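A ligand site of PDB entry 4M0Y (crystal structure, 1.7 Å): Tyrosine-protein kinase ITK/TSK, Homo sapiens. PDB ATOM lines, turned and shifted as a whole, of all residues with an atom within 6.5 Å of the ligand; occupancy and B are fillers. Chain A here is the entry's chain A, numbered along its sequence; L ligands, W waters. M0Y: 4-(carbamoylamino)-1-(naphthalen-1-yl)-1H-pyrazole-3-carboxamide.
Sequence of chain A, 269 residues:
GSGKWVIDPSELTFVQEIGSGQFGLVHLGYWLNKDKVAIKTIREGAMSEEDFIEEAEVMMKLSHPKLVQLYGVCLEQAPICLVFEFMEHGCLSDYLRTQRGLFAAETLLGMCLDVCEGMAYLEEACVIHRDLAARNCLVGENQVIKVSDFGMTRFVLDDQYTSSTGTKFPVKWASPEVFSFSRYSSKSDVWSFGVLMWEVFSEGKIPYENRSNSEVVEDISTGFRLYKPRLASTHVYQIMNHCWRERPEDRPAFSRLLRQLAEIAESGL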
ATOM      1  N   ILE A  18      13.349 -21.713   2.833  1.00  0.00           N
ATOM      2  CA  ILE A  18      13.718 -22.743   1.874  1.00  0.00           C
ATOM      3  C   ILE A  18      14.547 -22.225   0.694  1.00  0.00           C
ATOM      4  O   ILE A  18      15.168 -23.027  -0.010  1.00  0.00           O
ATOM      5  CB  ILE A  18      12.610 -23.783   1.545  1.00  0.00           C
ATOM      6  CG1 ILE A  18      11.275 -23.111   1.145  1.00  0.00           C
ATOM      7  CG2 ILE A  18      12.444 -24.740   2.741  1.00  0.00           C
ATOM      8  CD1 ILE A  18      10.126 -24.072   0.700  1.00  0.00           C
ATOM      9  N   GLY A  19      14.624 -20.901   0.573  1.00  0.00           N
ATOM     10  CA  GLY A  19      15.426 -20.245  -0.464  1.00  0.00           C
ATOM     11  C   GLY A  19      14.980 -18.841  -0.812  1.00  0.00           C
ATOM     12  O   GLY A  19      14.157 -18.247  -0.122  1.00  0.00           O
ATOM     13  N   SER A  20      15.552 -18.305  -1.905  1.00  0.00           N
ATOM     14  CA  SER A  20      15.277 -16.965  -2.411  1.00  0.00           C
ATOM     15  C   SER A  20      14.773 -17.061  -3.842  1.00  0.00           C
ATOM     16  O   SER A  20      15.410 -17.698  -4.690  1.00  0.00           O
ATOM     17  CB  SER A  20      16.527 -16.096  -2.364  1.00  0.00           C
ATOM     18  OG  SER A  20      16.897 -15.794  -1.024  1.00  0.00           O
ATOM     19  N   GLY A  21      13.610 -16.451  -4.082  1.00  0.00           N
ATOM     20  CA  GLY A  21      12.962 -16.403  -5.389  1.00  0.00           C
ATOM     21  C   GLY A  21      13.253 -15.113  -6.114  1.00  0.00           C
ATOM     22  O   GLY A  21      14.133 -14.346  -5.708  1.00  0.00           O
ATOM     23  N   GLN A  22      12.502 -14.858  -7.200  1.00  0.00           N
ATOM     24  CA  GLN A  22      12.651 -13.644  -8.016  1.00  0.00           C
ATOM     25  C   GLN A  22      12.242 -12.379  -7.243  1.00  0.00           C
ATOM     26  O   GLN A  22      12.875 -11.335  -7.396  1.00  0.00           O
ATOM     27  CB  GLN A  22      11.824 -13.791  -9.316  1.00  0.00           C
ATOM     28  CG  GLN A  22      11.971 -12.644 -10.333  1.00  0.00           C
ATOM     29  CD  GLN A  22      13.332 -12.575 -10.987  1.00  0.00           C
ATOM     30  OE1 GLN A  22      14.157 -11.706 -10.667  1.00  0.00           O
ATOM     31  NE2 GLN A  22      13.594 -13.463 -11.936  1.00  0.00           N
ATOM     32  N   GLY A  24      11.628 -12.245  -3.609  1.00  0.00           N
ATOM     33  CA  GLY A  24      11.952 -12.307  -2.191  1.00  0.00           C
ATOM     34  C   GLY A  24      12.112 -13.729  -1.689  1.00  0.00           C
ATOM     35  O   GLY A  24      12.262 -14.654  -2.478  1.00  0.00           O
ATOM     36  N   LEU A  25      12.055 -13.896  -0.368  1.00  0.00           N
ATOM     37  CA  LEU A  25      12.223 -15.181   0.303  1.00  0.00           C
ATOM     38  C   LEU A  25      11.032 -16.130   0.156  1.00  0.00           C
ATOM     39  O   LEU A  25       9.911 -15.696  -0.103  1.00  0.00           O
ATOM     40  CB  LEU A  25      12.511 -14.928   1.802  1.00  0.00           C
ATOM     41  CG  LEU A  25      13.951 -15.115   2.298  1.00  0.00           C
ATOM     42  CD1 LEU A  25      14.972 -14.400   1.428  1.00  0.00           C
ATOM     43  CD2 LEU A  25      14.080 -14.652   3.733  1.00  0.00           C
ATOM     44  N   VAL A  26      11.298 -17.429   0.303  1.00  0.00           N
ATOM     45  CA  VAL A  26      10.303 -18.495   0.285  1.00  0.00           C
ATOM     46  C   VAL A  26      10.497 -19.292   1.578  1.00  0.00           C
ATOM     47  O   VAL A  26      11.628 -19.700   1.885  1.00  0.00           O
ATOM     48  CB  VAL A  26      10.381 -19.415  -0.967  1.00  0.00           C
ATOM     49  CG1 VAL A  26       9.248 -20.455  -0.962  1.00  0.00           C
ATOM     50  CG2 VAL A  26      10.339 -18.599  -2.262  1.00  0.00           C
ATOM     51  N   VAL A  37       2.362 -25.326   4.301  1.00  0.00           N
ATOM     52  CA  VAL A  37       2.370 -24.427   3.139  1.00  0.00           C
ATOM     53  C   VAL A  37       3.772 -23.903   2.776  1.00  0.00           C
ATOM     54  O   VAL A  37       4.698 -23.968   3.588  1.00  0.00           O
ATOM     55  CB  VAL A  37       1.401 -23.216   3.365  1.00  0.00           C
ATOM     56  CG1 VAL A  37      -0.074 -23.640   3.401  1.00  0.00           C
ATOM     57  CG2 VAL A  37       1.777 -22.396   4.606  1.00  0.00           C
ATOM     58  N   ALA A  38       3.900 -23.373   1.552  1.00  0.00           N
ATOM     59  CA  ALA A  38       5.074 -22.622   1.089  1.00  0.00           C
ATOM     60  C   ALA A  38       4.579 -21.166   1.044  1.00  0.00           C
ATOM     61  O   ALA A  38       3.506 -20.901   0.490  1.00  0.00           O
ATOM     62  CB  ALA A  38       5.509 -23.067  -0.289  1.00  0.00           C
ATOM     63  N   LYS A  40       5.547 -17.268  -0.056  1.00  0.00           N
ATOM     64  CA  LYS A  40       6.455 -16.430  -0.846  1.00  0.00           C
ATOM     65  C   LYS A  40       6.233 -14.979  -0.488  1.00  0.00           C
ATOM     66  O   LYS A  40       5.129 -14.482  -0.677  1.00  0.00           O
ATOM     67  CB  LYS A  40       6.254 -16.651  -2.373  1.00  0.00           C
ATOM     68  CG  LYS A  40       6.565 -18.067  -2.844  1.00  0.00           C
ATOM     69  CD  LYS A  40       6.391 -18.234  -4.350  1.00  0.00           C
ATOM     70  CE  LYS A  40       7.710 -18.338  -5.081  1.00  0.00           C
ATOM     71  NZ  LYS A  40       7.504 -18.439  -6.550  1.00  0.00           N
ATOM     72  N   VAL A  68      -0.425 -26.179  -9.053  1.00  0.00           N
ATOM     73  CA  VAL A  68      -0.077 -25.834  -7.675  1.00  0.00           C
ATOM     74  C   VAL A  68      -1.178 -24.885  -7.153  1.00  0.00           C
ATOM     75  O   VAL A  68      -1.456 -23.856  -7.774  1.00  0.00           O
ATOM     76  CB  VAL A  68       1.343 -25.188  -7.558  1.00  0.00           C
ATOM     77  CG1 VAL A  68       1.623 -24.682  -6.139  1.00  0.00           C
ATOM     78  CG2 VAL A  68       2.439 -26.170  -8.004  1.00  0.00           C
ATOM     79  N   PHE A  84       0.944 -20.925  -0.781  1.00  0.00           N
ATOM     80  CA  PHE A  84       0.762 -22.024  -1.730  1.00  0.00           C
ATOM     81  C   PHE A  84       0.820 -23.386  -1.083  1.00  0.00           C
ATOM     82  O   PHE A  84       1.455 -23.581  -0.021  1.00  0.00           O
ATOM     83  CB  PHE A  84       1.901 -21.993  -2.767  1.00  0.00           C
ATOM     84  CG  PHE A  84       2.041 -20.764  -3.630  1.00  0.00           C
ATOM     85  CD1 PHE A  84       1.481 -20.714  -4.900  1.00  0.00           C
ATOM     86  CD2 PHE A  84       2.775 -19.660  -3.190  1.00  0.00           C
ATOM     87  CE1 PHE A  84       1.628 -19.584  -5.710  1.00  0.00           C
ATOM     88  CE2 PHE A  84       2.913 -18.521  -3.995  1.00  0.00           C
ATOM     89  CZ  PHE A  84       2.345 -18.495  -5.250  1.00  0.00           C
ATOM     90  N   GLU A  85       0.274 -24.378  -1.823  1.00  0.00           N
ATOM     91  CA  GLU A  85       0.386 -25.801  -1.557  1.00  0.00           C
ATOM     92  C   GLU A  85       1.910 -26.122  -1.489  1.00  0.00           C
ATOM     93  O   GLU A  85       2.687 -25.638  -2.319  1.00  0.00           O
ATOM     94  CB  GLU A  85      -0.273 -26.516  -2.754  1.00  0.00           C
ATOM     95  CG  GLU A  85      -0.036 -28.007  -2.872  1.00  0.00           C
ATOM     96  CD  GLU A  85      -0.665 -28.680  -4.073  1.00  0.00           C
ATOM     97  OE1 GLU A  85      -1.356 -28.003  -4.872  1.00  0.00           O
ATOM     98  OE2 GLU A  85      -0.518 -29.918  -4.171  1.00  0.00           O
ATOM     99  N   PHE A  86       2.339 -26.874  -0.462  1.00  0.00           N
ATOM    100  CA  PHE A  86       3.755 -27.228  -0.320  1.00  0.00           C
ATOM    101  C   PHE A  86       4.125 -28.393  -1.246  1.00  0.00           C
ATOM    102  O   PHE A  86       3.458 -29.430  -1.212  1.00  0.00           O
ATOM    103  CB  PHE A  86       4.097 -27.573   1.135  1.00  0.00           C
ATOM    104  CG  PHE A  86       5.528 -28.034   1.316  1.00  0.00           C
ATOM    105  CD1 PHE A  86       6.586 -27.150   1.118  1.00  0.00           C
ATOM    106  CD2 PHE A  86       5.821 -29.340   1.701  1.00  0.00           C
ATOM    107  CE1 PHE A  86       7.914 -27.567   1.289  1.00  0.00           C
ATOM    108  CE2 PHE A  86       7.149 -29.757   1.872  1.00  0.00           C
ATOM    109  CZ  PHE A  86       8.186 -28.861   1.671  1.00  0.00           C
ATOM    110  N   MET A  87       5.196 -28.227  -2.038  1.00  0.00           N
ATOM    111  CA  MET A  87       5.679 -29.250  -2.985  1.00  0.00           C
ATOM    112  C   MET A  87       7.055 -29.741  -2.463  1.00  0.00           C
ATOM    113  O   MET A  87       8.060 -29.051  -2.593  1.00  0.00           O
ATOM    114  CB  MET A  87       5.779 -28.660  -4.408  1.00  0.00           C
ATOM    115  CG  MET A  87       4.456 -28.101  -4.930  1.00  0.00           C
ATOM    116  SD  MET A  87       3.184 -29.369  -5.180  1.00  0.00           S
ATOM    117  CE  MET A  87       3.885 -30.263  -6.639  1.00  0.00           C
ATOM    118  N   GLU A  88       7.056 -30.936  -1.871  1.00  0.00           N
ATOM    119  CA  GLU A  88       8.242 -31.534  -1.208  1.00  0.00           C
ATOM    120  C   GLU A  88       9.593 -31.544  -1.948  1.00  0.00           C
ATOM    121  O   GLU A  88      10.628 -31.431  -1.282  1.00  0.00           O
ATOM    122  CB  GLU A  88       7.918 -32.880  -0.536  1.00  0.00           C
ATOM    123  CG  GLU A  88       7.777 -34.062  -1.465  1.00  0.00           C
ATOM    124  CD  GLU A  88       7.607 -35.384  -0.741  1.00  0.00           C
ATOM    125  OE1 GLU A  88       8.621 -35.921  -0.238  1.00  0.00           O
ATOM    126  OE2 GLU A  88       6.453 -35.877  -0.671  1.00  0.00           O
ATOM    127  N   HIS A  89       9.585 -31.690  -3.287  1.00  0.00           N
ATOM    128  CA  HIS A  89      10.837 -31.778  -4.053  1.00  0.00           C
ATOM    129  C   HIS A  89      11.332 -30.505  -4.780  1.00  0.00           C
ATOM    130  O   HIS A  89      12.345 -30.562  -5.470  1.00  0.00           O
ATOM    131  CB  HIS A  89      10.867 -33.041  -4.934  1.00  0.00           C
ATOM    132  CG  HIS A  89      10.749 -34.318  -4.164  1.00  0.00           C
ATOM    133  ND1 HIS A  89       9.616 -35.102  -4.250  1.00  0.00           N
ATOM    134  CD2 HIS A  89      11.618 -34.893  -3.305  1.00  0.00           C
ATOM    135  CE1 HIS A  89       9.834 -36.143  -3.462  1.00  0.00           C
ATOM    136  NE2 HIS A  89      11.020 -36.057  -2.854  1.00  0.00           N
ATOM    137  N   GLY A  90      10.640 -29.383  -4.581  1.00  0.00           N
ATOM    138  CA  GLY A  90      11.042 -28.103  -5.160  1.00  0.00           C
ATOM    139  C   GLY A  90      10.888 -27.969  -6.663  1.00  0.00           C
ATOM    140  O   GLY A  90      10.062 -28.661  -7.269  1.00  0.00           O
ATOM    141  N   CYS A  91      11.652 -27.036  -7.269  1.00  0.00           N
ATOM    142  CA  CYS A  91      11.545 -26.737  -8.709  1.00  0.00           C
ATOM    143  C   CYS A  91      12.001 -27.872  -9.621  1.00  0.00           C
ATOM    144  O   CYS A  91      13.004 -28.528  -9.354  1.00  0.00           O
ATOM    145  CB  CYS A  91      12.221 -25.413  -9.050  1.00  0.00           C
ATOM    146  SG  CYS A  91      11.609 -24.007  -8.089  1.00  0.00           S
ATOM    147  N   ARG A 135      11.548 -24.099 -14.632  1.00  0.00           N
ATOM    148  CA  ARG A 135      11.747 -23.322 -13.402  1.00  0.00           C
ATOM    149  C   ARG A 135      10.420 -22.960 -12.697  1.00  0.00           C
ATOM    150  O   ARG A 135      10.435 -22.648 -11.500  1.00  0.00           O
ATOM    151  CB  ARG A 135      12.642 -22.086 -13.653  1.00  0.00           C
ATOM    152  CG  ARG A 135      12.051 -21.127 -14.661  1.00  0.00           C
ATOM    153  CD  ARG A 135      12.788 -19.798 -14.747  1.00  0.00           C
ATOM    154  NE  ARG A 135      12.027 -18.855 -15.578  1.00  0.00           N
ATOM    155  CZ  ARG A 135      12.058 -18.830 -16.905  1.00  0.00           C
ATOM    156  NH1 ARG A 135      12.817 -19.687 -17.567  1.00  0.00           N
ATOM    157  NH2 ARG A 135      11.316 -17.953 -17.580  1.00  0.00           N
ATOM    158  N   ASN A 136       9.270 -22.966 -13.446  1.00  0.00           N
ATOM    159  CA  ASN A 136       7.937 -22.647 -12.913  1.00  0.00           C
ATOM    160  C   ASN A 136       7.097 -23.889 -12.589  1.00  0.00           C
ATOM    161  O   ASN A 136       5.932 -23.738 -12.214  1.00  0.00           O
ATOM    162  CB  ASN A 136       7.184 -21.723 -13.858  1.00  0.00           C
ATOM    163  CG  ASN A 136       7.573 -20.274 -13.713  1.00  0.00           C
ATOM    164  OD1 ASN A 136       7.851 -19.773 -12.604  1.00  0.00           O
ATOM    165  ND2 ASN A 136       7.587 -19.561 -14.816  1.00  0.00           N
ATOM    166  N   LEU A 138       6.691 -27.538 -10.352  1.00  0.00           N
ATOM    167  CA  LEU A 138       7.120 -28.065  -9.054  1.00  0.00           C
ATOM    168  C   LEU A 138       6.955 -29.575  -8.984  1.00  0.00           C
ATOM    169  O   LEU A 138       6.088 -30.117  -9.663  1.00  0.00           O
ATOM    170  CB  LEU A 138       6.359 -27.377  -7.911  1.00  0.00           C
ATOM    171  CG  LEU A 138       6.754 -25.937  -7.484  1.00  0.00           C
ATOM    172  CD1 LEU A 138       8.145 -25.854  -6.821  1.00  0.00           C
ATOM    173  CD2 LEU A 138       6.519 -24.897  -8.556  1.00  0.00           C
ATOM    174  N   VAL A 139       7.775 -30.242  -8.154  1.00  0.00           N
ATOM    175  CA  VAL A 139       7.793 -31.708  -7.999  1.00  0.00           C
ATOM    176  C   VAL A 139       7.236 -32.042  -6.602  1.00  0.00           C
ATOM    177  O   VAL A 139       7.778 -31.563  -5.602  1.00  0.00           O
ATOM    178  CB  VAL A 139       9.227 -32.293  -8.186  1.00  0.00           C
ATOM    179  CG1 VAL A 139       9.218 -33.822  -8.205  1.00  0.00           C
ATOM    180  CG2 VAL A 139       9.899 -31.748  -9.445  1.00  0.00           C
ATOM    181  N   SER A 148       2.870 -23.958 -12.035  1.00  0.00           N
ATOM    182  CA  SER A 148       2.649 -22.835 -11.118  1.00  0.00           C
ATOM    183  C   SER A 148       2.957 -21.490 -11.819  1.00  0.00           C
ATOM    184  O   SER A 148       3.535 -21.466 -12.911  1.00  0.00           O
ATOM    185  CB  SER A 148       3.526 -23.010  -9.873  1.00  0.00           C
ATOM    186  OG  SER A 148       3.269 -21.989  -8.917  1.00  0.00           O
ATOM    187  N   ASP A 149       2.535 -20.370 -11.194  1.00  0.00           N
ATOM    188  CA  ASP A 149       2.796 -19.000 -11.676  1.00  0.00           C
ATOM    189  C   ASP A 149       2.116 -18.582 -12.992  1.00  0.00           C
ATOM    190  O   ASP A 149       2.549 -17.601 -13.626  1.00  0.00           O
ATOM    191  CB  ASP A 149       4.297 -18.704 -11.714  1.00  0.00           C
ATOM    192  CG  ASP A 149       4.970 -18.611 -10.358  1.00  0.00           C
ATOM    193  OD1 ASP A 149       4.506 -19.291  -9.414  1.00  0.00           O
ATOM    194  OD2 ASP A 149       5.992 -17.906 -10.253  1.00  0.00           O
HETATM  195  C1  M0Y L   1      13.569 -20.250  -3.969  1.00  0.00           C
HETATM  196  C2  M0Y L   1      13.020 -21.196  -3.058  1.00  0.00           C
HETATM  197  C3  M0Y L   1      11.846 -21.860  -3.366  1.00  0.00           C
HETATM  198  C4  M0Y L   1      11.164 -21.607  -4.614  1.00  0.00           C
HETATM  199  C5  M0Y L   1      11.727 -20.624  -5.516  1.00  0.00           C
HETATM  200  C6  M0Y L   1      12.949 -19.975  -5.169  1.00  0.00           C
HETATM  201  C7  M0Y L   1      11.052 -20.303  -6.745  1.00  0.00           C
HETATM  202  C8  M0Y L   1       9.864 -20.918  -7.078  1.00  0.00           C
HETATM  203  C9  M0Y L   1       9.292 -21.897  -6.225  1.00  0.00           C
HETATM  204  C10 M0Y L   1       9.931 -22.248  -5.020  1.00  0.00           C
HETATM  205  N1  M0Y L   1       9.335 -23.322  -4.267  1.00  0.00           N
HETATM  206  C11 M0Y L   1      10.046 -24.354  -3.623  1.00  0.00           C
HETATM  207  C12 M0Y L   1       9.085 -25.166  -3.049  1.00  0.00           C
HETATM  208  C13 M0Y L   1       7.812 -24.560  -3.386  1.00  0.00           C
HETATM  209  N2  M0Y L   1       8.005 -23.447  -4.114  1.00  0.00           N
HETATM  210  C14 M0Y L   1       6.476 -25.004  -2.957  1.00  0.00           C
HETATM  211  O1  M0Y L   1       6.388 -25.910  -2.143  1.00  0.00           O
HETATM  212  N3  M0Y L   1       5.328 -24.346  -3.440  1.00  0.00           N
HETATM  213  N4  M0Y L   1       9.236 -26.349  -2.323  1.00  0.00           N
HETATM  214  C15 M0Y L   1      10.497 -26.944  -1.949  1.00  0.00           C
HETATM  215  O2  M0Y L   1      11.625 -26.460  -2.198  1.00  0.00           O
HETATM  216  N5  M0Y L   1      10.399 -28.142  -1.244  1.00  0.00           N
HETATM  217  O   HOH W   1       4.984 -22.033  -4.943  1.00  0.00           O
HETATM  218  O   HOH W   2       7.698 -20.148  -9.447  1.00  0.00           O
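N of Met 87 sits at hydrogen-bond distance from O1 of the ligand, 2.6 Å away. O of Met 87 is in hydrogen-bond range of N5 of the ligand (2.8 Å). O of Glu 85 sits at hydrogen-bond distance from N3 of the ligand, at 3.1 Å. The backbone carbonyl oxygen (O) of Glu 88 lies within hydrogen-bond range of a nitrogen (N5) of the ligand.
The backbone carbonyl oxygen of Ala 38 is in hydrogen-bond range of the backbone NH of Phe 84, 2.9 Å away. O of Gly 90 sits at hydrogen-bond distance from N of Val 139 (2.9 Å). The backbone carbonyl oxygen (O) of Gly 19 sits at hydrogen-bond distance from the backbone NH (N) of Val 26. The backbone carbonyl oxygen of Val 26 is in hydrogen-bond range of the backbone NH of Ile 18 (2.8 Å).
Residues that only touch the ligand: Ile 18, Gly 19, Ser 20, Gly 21, Val 26, Ala 38, Lys 40, Phe 86, Gly 90, Cys 91 and Leu 138. Hydrophobic or aromatic side chains that line the ligand: Ile 18, Val 26, Ala 38, Phe 86, Met 87 and Leu 138. 14 residues have an atom within 4 Å of the ligand: Ile 18, Gly 19, Ser 20, Gly 21, Val 26, Ala 38, Lys 40, Glu 85, Phe 86, Met 87, Glu 88, Gly 90, Cys 91 and Leu 138.
Water W2 lies within hydrogen-bond range of the side-chain carboxylate of Asp 149 (2.9 Å), the side-chain amide oxygen of Asn 136 (3.2 Å) and the side-chain amino group of Lys 40 (3.4 Å).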
